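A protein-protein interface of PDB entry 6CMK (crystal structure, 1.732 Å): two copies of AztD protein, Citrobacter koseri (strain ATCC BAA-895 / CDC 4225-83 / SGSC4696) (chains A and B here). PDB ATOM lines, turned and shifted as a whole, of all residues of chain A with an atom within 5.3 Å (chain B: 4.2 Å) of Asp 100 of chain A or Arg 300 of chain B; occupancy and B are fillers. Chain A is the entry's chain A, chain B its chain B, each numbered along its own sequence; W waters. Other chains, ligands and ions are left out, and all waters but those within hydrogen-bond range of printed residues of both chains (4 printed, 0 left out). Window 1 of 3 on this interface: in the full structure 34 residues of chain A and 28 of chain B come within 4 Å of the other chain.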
ATOM      1  N   PHE A  98      -2.777  13.332   5.850  1.00  0.00           N
ATOM      2  CA  PHE A  98      -2.629  12.113   5.073  1.00  0.00           C
ATOM      3  C   PHE A  98      -2.009  10.986   5.883  1.00  0.00           C
ATOM      4  O   PHE A  98      -1.333  11.201   6.897  1.00  0.00           O
ATOM      5  CB  PHE A  98      -1.778  12.356   3.832  1.00  0.00           C
ATOM      6  CG  PHE A  98      -2.384  13.337   2.879  1.00  0.00           C
ATOM      7  CD1 PHE A  98      -3.364  12.940   1.982  1.00  0.00           C
ATOM      8  CD2 PHE A  98      -1.981  14.668   2.897  1.00  0.00           C
ATOM      9  CE1 PHE A  98      -3.926  13.851   1.081  1.00  0.00           C
ATOM     10  CE2 PHE A  98      -2.540  15.575   2.009  1.00  0.00           C
ATOM     11  CZ  PHE A  98      -3.513  15.172   1.114  1.00  0.00           C
ATOM     12  N   HIS A  99      -2.283   9.768   5.423  1.00  0.00           N
ATOM     13  CA  HIS A  99      -1.614   8.565   5.895  1.00  0.00           C
ATOM     14  C   HIS A  99      -0.948   7.881   4.710  1.00  0.00           C
ATOM     15  O   HIS A  99      -1.597   7.641   3.686  1.00  0.00           O
ATOM     16  CB  HIS A  99      -2.597   7.608   6.565  1.00  0.00           C
ATOM     17  CG  HIS A  99      -3.302   8.196   7.742  1.00  0.00           C
ATOM     18  ND1 HIS A  99      -2.690   8.363   8.965  1.00  0.00           N
ATOM     19  CD2 HIS A  99      -4.567   8.656   7.885  1.00  0.00           C
ATOM     20  CE1 HIS A  99      -3.548   8.904   9.811  1.00  0.00           C
ATOM     21  NE2 HIS A  99      -4.694   9.090   9.181  1.00  0.00           N
ATOM     22  N   ASP A 100       0.336   7.560   4.869  1.00  0.00           N
ATOM     23  CA  ASP A 100       1.167   6.961   3.822  1.00  0.00           C
ATOM     24  C   ASP A 100       1.034   5.445   3.900  1.00  0.00           C
ATOM     25  O   ASP A 100       1.638   4.806   4.763  1.00  0.00           O
ATOM     26  CB  ASP A 100       2.618   7.397   4.010  1.00  0.00           C
ATOM     27  CG  ASP A 100       3.551   6.868   2.930  1.00  0.00           C
ATOM     28  OD1 ASP A 100       3.121   6.044   2.101  1.00  0.00           O
ATOM     29  OD2 ASP A 100       4.731   7.297   2.922  1.00  0.00           O
ATOM     30  N   HIS A 101       0.271   4.857   2.977  1.00  0.00           N
ATOM     31  CA  HIS A 101      -0.024   3.429   3.008  1.00  0.00           C
ATOM     32  C   HIS A 101       0.619   2.673   1.845  1.00  0.00           C
ATOM     33  O   HIS A 101       0.092   1.658   1.381  1.00  0.00           O
ATOM     34  CB  HIS A 101      -1.534   3.225   3.058  1.00  0.00           C
ATOM     35  CG  HIS A 101      -2.109   3.502   4.415  1.00  0.00           C
ATOM     36  ND1 HIS A 101      -3.454   3.420   4.696  1.00  0.00           N
ATOM     37  CD2 HIS A 101      -1.502   3.844   5.578  1.00  0.00           C
ATOM     38  CE1 HIS A 101      -3.654   3.706   5.973  1.00  0.00           C
ATOM     39  NE2 HIS A 101      -2.485   3.967   6.530  1.00  0.00           N
ATOM     40  N   GLY A 102       1.777   3.145   1.395  1.00  0.00           N
ATOM     41  CA  GLY A 102       2.561   2.428   0.408  1.00  0.00           C
ATOM     42  C   GLY A 102       2.036   2.596  -1.000  1.00  0.00           C
ATOM     43  O   GLY A 102       2.415   3.536  -1.701  1.00  0.00           O
ATOM     44  N   HIS A 104      -1.034   3.305  -1.701  1.00  0.00           N
ATOM     45  CA  HIS A 104      -2.104   4.288  -1.682  1.00  0.00           C
ATOM     46  C   HIS A 104      -1.895   5.210  -0.492  1.00  0.00           C
ATOM     47  O   HIS A 104      -1.063   4.955   0.383  1.00  0.00           O
ATOM     48  CB  HIS A 104      -3.479   3.620  -1.609  1.00  0.00           C
ATOM     49  CG  HIS A 104      -3.641   2.705  -0.435  1.00  0.00           C
ATOM     50  ND1 HIS A 104      -2.978   1.501  -0.334  1.00  0.00           N
ATOM     51  CD2 HIS A 104      -4.386   2.819   0.690  1.00  0.00           C
ATOM     52  CE1 HIS A 104      -3.309   0.912   0.801  1.00  0.00           C
ATOM     53  NE2 HIS A 104      -4.163   1.690   1.440  1.00  0.00           N
ATOM     54  N   ALA A 105      -2.658   6.300  -0.477  1.00  0.00           N
ATOM     55  CA  ALA A 105      -2.688   7.225   0.640  1.00  0.00           C
ATOM     56  C   ALA A 105      -4.137   7.423   1.048  1.00  0.00           C
ATOM     57  O   ALA A 105      -5.045   7.347   0.212  1.00  0.00           O
ATOM     58  CB  ALA A 105      -2.051   8.580   0.287  1.00  0.00           C
ATOM     59  N   SER B 260       3.783   3.094   8.593  1.00  0.00           N
ATOM     60  CA  SER B 260       2.492   2.678   8.070  1.00  0.00           C
ATOM     61  C   SER B 260       2.606   1.807   6.821  1.00  0.00           C
ATOM     62  O   SER B 260       1.577   1.464   6.228  1.00  0.00           O
ATOM     63  CB  SER B 260       1.627   3.922   7.759  1.00  0.00           C
ATOM     64  OG  SER B 260       2.395   4.892   7.064  1.00  0.00           O
ATOM     65  N   THR B 261       3.814   1.448   6.402  1.00  0.00           N
ATOM     66  CA  THR B 261       4.014   0.545   5.282  1.00  0.00           C
ATOM     67  C   THR B 261       5.350  -0.160   5.477  1.00  0.00           C
ATOM     68  O   THR B 261       6.305   0.449   5.953  1.00  0.00           O
ATOM     69  CB  THR B 261       3.962   1.307   3.947  1.00  0.00           C
ATOM     70  OG1 THR B 261       3.969   0.373   2.868  1.00  0.00           O
ATOM     71  CG2 THR B 261       5.135   2.248   3.783  1.00  0.00           C
ATOM     72  N   ASN B 274       8.507   2.953   6.363  1.00  0.00           N
ATOM     73  CA  ASN B 274       8.597   4.401   6.352  1.00  0.00           C
ATOM     74  C   ASN B 274       8.673   4.894   7.796  1.00  0.00           C
ATOM     75  O   ASN B 274       8.402   4.163   8.748  1.00  0.00           O
ATOM     76  CB  ASN B 274       7.399   5.023   5.635  1.00  0.00           C
ATOM     77  CG  ASN B 274       6.094   4.827   6.393  1.00  0.00           C
ATOM     78  OD1 ASN B 274       5.819   3.750   6.903  1.00  0.00           O
ATOM     79  ND2 ASN B 274       5.307   5.894   6.507  1.00  0.00           N
ATOM     80  N   PRO B 277       7.738  10.513   5.384  1.00  0.00           N
ATOM     81  CA  PRO B 277       7.916  10.179   3.968  1.00  0.00           C
ATOM     82  C   PRO B 277       9.346  10.226   3.465  1.00  0.00           C
ATOM     83  O   PRO B 277       9.632   9.544   2.468  1.00  0.00           O
ATOM     84  CB  PRO B 277       7.044  11.215   3.257  1.00  0.00           C
ATOM     85  CG  PRO B 277       6.946  12.342   4.216  1.00  0.00           C
ATOM     86  CD  PRO B 277       6.888  11.695   5.566  1.00  0.00           C
ATOM     87  N   LEU B 296      16.483   9.735   3.880  1.00  0.00           N
ATOM     88  CA  LEU B 296      16.479   9.717   2.421  1.00  0.00           C
ATOM     89  C   LEU B 296      16.729  11.113   1.866  1.00  0.00           C
ATOM     90  O   LEU B 296      16.421  12.105   2.527  1.00  0.00           O
ATOM     91  CB  LEU B 296      15.139   9.206   1.899  1.00  0.00           C
ATOM     92  CG  LEU B 296      14.712   7.810   2.343  1.00  0.00           C
ATOM     93  CD1 LEU B 296      13.307   7.522   1.839  1.00  0.00           C
ATOM     94  CD2 LEU B 296      15.702   6.750   1.868  1.00  0.00           C
ATOM     95  N   THR B 298      15.191  12.649  -0.662  1.00  0.00           N
ATOM     96  CA  THR B 298      13.868  13.217  -0.873  1.00  0.00           C
ATOM     97  C   THR B 298      12.863  12.133  -0.486  1.00  0.00           C
ATOM     98  O   THR B 298      13.237  11.074   0.035  1.00  0.00           O
ATOM     99  CB  THR B 298      13.675  13.714  -2.320  1.00  0.00           C
ATOM    100  OG1 THR B 298      14.003  12.677  -3.242  1.00  0.00           O
ATOM    101  CG2 THR B 298      14.563  14.912  -2.616  1.00  0.00           C
ATOM    102  N   ARG B 299      11.579  12.408  -0.702  1.00  0.00           N
ATOM    103  CA  ARG B 299      10.551  11.492  -0.224  1.00  0.00           C
ATOM    104  C   ARG B 299      10.560  10.178  -1.001  1.00  0.00           C
ATOM    105  O   ARG B 299      10.847  10.125  -2.198  1.00  0.00           O
ATOM    106  CB  ARG B 299       9.162  12.123  -0.306  1.00  0.00           C
ATOM    107  CG  ARG B 299       8.969  13.269   0.697  1.00  0.00           C
ATOM    108  CD  ARG B 299       7.654  14.004   0.482  1.00  0.00           C
ATOM    109  NE  ARG B 299       7.692  14.740  -0.770  1.00  0.00           N
ATOM    110  CZ  ARG B 299       6.771  15.609  -1.172  1.00  0.00           C
ATOM    111  NH1 ARG B 299       5.714  15.875  -0.413  1.00  0.00           N
ATOM    112  NH2 ARG B 299       6.918  16.216  -2.346  1.00  0.00           N
ATOM    113  N   ARG B 300      10.175   9.126  -0.295  1.00  0.00           N
ATOM    114  CA  ARG B 300      10.115   7.776  -0.838  1.00  0.00           C
ATOM    115  C   ARG B 300       8.958   7.630  -1.815  1.00  0.00           C
ATOM    116  O   ARG B 300       7.818   7.974  -1.498  1.00  0.00           O
ATOM    117  CB  ARG B 300       9.940   6.787   0.315  1.00  0.00           C
ATOM    118  CG  ARG B 300       9.895   5.310  -0.082  1.00  0.00           C
ATOM    119  CD  ARG B 300       9.194   4.466   0.998  1.00  0.00           C
ATOM    120  NE  ARG B 300       7.780   4.244   0.675  1.00  0.00           N
ATOM    121  CZ  ARG B 300       6.749   4.862   1.246  1.00  0.00           C
ATOM    122  NH1 ARG B 300       6.923   5.756   2.215  1.00  0.00           N
ATOM    123  NH2 ARG B 300       5.522   4.575   0.842  1.00  0.00           N
ATOM    124  N   VAL B 301       9.249   7.060  -2.981  1.00  0.00           N
ATOM    125  CA  VAL B 301       8.232   6.647  -3.942  1.00  0.00           C
ATOM    126  C   VAL B 301       7.910   5.162  -3.798  1.00  0.00           C
ATOM    127  O   VAL B 301       6.742   4.768  -3.787  1.00  0.00           O
ATOM    128  CB  VAL B 301       8.697   6.979  -5.379  1.00  0.00           C
ATOM    129  CG1 VAL B 301       7.750   6.377  -6.428  1.00  0.00           C
ATOM    130  CG2 VAL B 301       8.777   8.504  -5.583  1.00  0.00           C
ATOM    131  N   HIS B 302       8.947   4.335  -3.689  1.00  0.00           N
ATOM    132  CA  HIS B 302       8.787   2.886  -3.611  1.00  0.00           C
ATOM    133  C   HIS B 302      10.011   2.281  -2.938  1.00  0.00           C
ATOM    134  O   HIS B 302      11.099   2.847  -2.976  1.00  0.00           O
ATOM    135  CB  HIS B 302       8.593   2.276  -5.010  1.00  0.00           C
ATOM    136  CG  HIS B 302       8.062   0.884  -4.993  1.00  0.00           C
ATOM    137  ND1 HIS B 302       8.561  -0.113  -5.803  1.00  0.00           N
ATOM    138  CD2 HIS B 302       7.070   0.319  -4.269  1.00  0.00           C
ATOM    139  CE1 HIS B 302       7.891  -1.229  -5.587  1.00  0.00           C
ATOM    140  NE2 HIS B 302       6.983  -0.996  -4.658  1.00  0.00           N
ATOM    141  N   PHE B 303       9.831   1.120  -2.319  1.00  0.00           N
ATOM    142  CA  PHE B 303      10.996   0.375  -1.873  1.00  0.00           C
ATOM    143  C   PHE B 303      10.716  -1.120  -1.937  1.00  0.00           C
ATOM    144  O   PHE B 303       9.565  -1.562  -1.875  1.00  0.00           O
ATOM    145  CB  PHE B 303      11.500   0.833  -0.477  1.00  0.00           C
ATOM    146  CG  PHE B 303      10.504   0.784   0.688  1.00  0.00           C
ATOM    147  CD1 PHE B 303       9.225   0.259   0.610  1.00  0.00           C
ATOM    148  CD2 PHE B 303      10.920   1.316   1.908  1.00  0.00           C
ATOM    149  CE1 PHE B 303       8.390   0.251   1.747  1.00  0.00           C
ATOM    150  CE2 PHE B 303      10.099   1.311   3.033  1.00  0.00           C
ATOM    151  CZ  PHE B 303       8.840   0.771   2.954  1.00  0.00           C
ATOM    152  N   VAL B 315      15.489   1.836  -2.427  1.00  0.00           N
ATOM    153  CA  VAL B 315      14.464   2.854  -2.262  1.00  0.00           C
ATOM    154  C   VAL B 315      14.542   3.783  -3.460  1.00  0.00           C
ATOM    155  O   VAL B 315      15.614   4.306  -3.767  1.00  0.00           O
ATOM    156  CB  VAL B 315      14.640   3.662  -0.960  1.00  0.00           C
ATOM    157  CG1 VAL B 315      13.491   4.643  -0.806  1.00  0.00           C
ATOM    158  CG2 VAL B 315      14.726   2.748   0.238  1.00  0.00           C
ATOM    159  N   PHE B 316      13.418   3.968  -4.135  1.00  0.00           N
ATOM    160  CA  PHE B 316      13.307   4.952  -5.198  1.00  0.00           C
ATOM    161  C   PHE B 316      12.700   6.208  -4.604  1.00  0.00           C
ATOM    162  O   PHE B 316      11.690   6.135  -3.897  1.00  0.00           O
ATOM    163  CB  PHE B 316      12.442   4.444  -6.347  1.00  0.00           C
ATOM    164  CG  PHE B 316      12.605   5.256  -7.593  1.00  0.00           C
ATOM    165  CD1 PHE B 316      11.806   6.348  -7.833  1.00  0.00           C
ATOM    166  CD2 PHE B 316      13.620   4.956  -8.486  1.00  0.00           C
ATOM    167  CE1 PHE B 316      11.998   7.113  -8.958  1.00  0.00           C
ATOM    168  CE2 PHE B 316      13.809   5.711  -9.622  1.00  0.00           C
ATOM    169  CZ  PHE B 316      12.992   6.793  -9.848  1.00  0.00           C
ATOM    170  N   MET B 344       6.083  13.543  -4.922  1.00  0.00           N
ATOM    171  CA  MET B 344       5.038  12.881  -4.156  1.00  0.00           C
ATOM    172  C   MET B 344       3.879  13.809  -3.814  1.00  0.00           C
ATOM    173  O   MET B 344       2.890  13.359  -3.222  1.00  0.00           O
ATOM    174  CB  MET B 344       5.642  12.256  -2.889  1.00  0.00           C
ATOM    175  CG  MET B 344       6.470  11.016  -3.195  1.00  0.00           C
ATOM    176  SD  MET B 344       5.452   9.700  -3.884  1.00  0.00           S
ATOM    177  CE  MET B 344       4.585   9.159  -2.424  1.00  0.00           C
HETATM  178  O   HOH W   1       6.409   9.156   0.735  1.00  0.00           O
HETATM  179  O   HOH W   2       1.754   7.698   7.387  1.00  0.00           O
HETATM  180  O   HOH W   3       5.412   8.469   5.491  1.00  0.00           O
HETATM  181  O   HOH W   4       4.792   2.779  -2.891  1.00  0.00           O
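Hydrophobic or aromatic side chains of chain A that line the printed part of chain B: His 101.
Among the printed residues, Asp or Glu carboxylates within 4 Å of a Lys or Arg side-chain nitrogen of the other chain: Asp 100 of chain A with Arg 300 of chain B.
Among the printed residues, merely in contact across the chains: Gly 102 of chain A with Thr 261 of chain B (3.5 Å), Gly 102 of chain A with Arg 300 of chain B (3.7 Å), His 101 of chain A with Ser 260 of chain B (3.8 Å) and Asp 100 of chain A with Asn 274 of chain B (3.9 Å).
The side-chain carboxylate of Asp 100 of chain A is in salt-bridge range of the guanidinium group of Arg 300 of chain B (2.8 Å).
The side-chain hydroxyl of Ser 260 of chain B lies within hydrogen-bond range of the backbone carbonyl oxygen of Asp 100 of chain A, 2.4 Å away.
Water W4 bridges the backbone carbonyl oxygen of Gly 102 of chain A and the backbone carbonyl oxygen of Val 301 of chain B.
Water W3 lies within hydrogen-bond range of ND2 of Asn 274 of chain B and OD2 of Asp 100 of chain A.
Water W1 lies within hydrogen-bond range of the backbone carbonyl oxygen (O) of Arg 300 of chain B (2.9 Å) and the side-chain carboxylate (OD2) of Asp 100 of chain A (3.3 Å).
Water W2 lies within hydrogen-bond range of N of Asp 100 of chain A (2.9 Å) and OG of Ser 260 of chain B (2.9 Å).
No position is printed for both chains.
N of Arg 300 of chain B is in hydrogen-bond range of O of Pro 277 of chain B (2.8 Å).
OD1 of Asn 274 of chain B sits at hydrogen-bond distance from N of Ser 260 of chain B.
The side-chain carboxylate (OD1) of Asp 100 of chain A lies within hydrogen-bond range of the backbone NH (N) of Gly 102 of chain A, 3.3 Å away.
The side-chain amide oxygen of Asn 274 of chain B sits at hydrogen-bond distance from the backbone NH of Thr 261 of chain B, 3.1 Å away.
Arg 300 of chain B touches just these residues of chain A: Asp 100 and Gly 102.
Of the printed residues of chain A, Asn 274 of chain B touches Asp 100 (3.9 Å).
Printed residues of chain A within 4 Å of Ser 260 of chain B: Asp 100 (2.4 Å) and His 101 (3.8 Å).
Printed residues of chain B within 4 Å of His 101 of chain A: Ser 260.
Of the printed residues of chain B, Gly 102 of chain A touches Thr 261 (3.5 Å) and Arg 300 (3.7 Å).
Of the printed residues of chain A, Thr 261 of chain B touches Gly 102.
Ala 105 of chain A touches none of the printed residues of chain B.
The nearest printed residue of chain B that does not touch His 101 of chain A is Thr 261 of chain B (4.2 Å).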
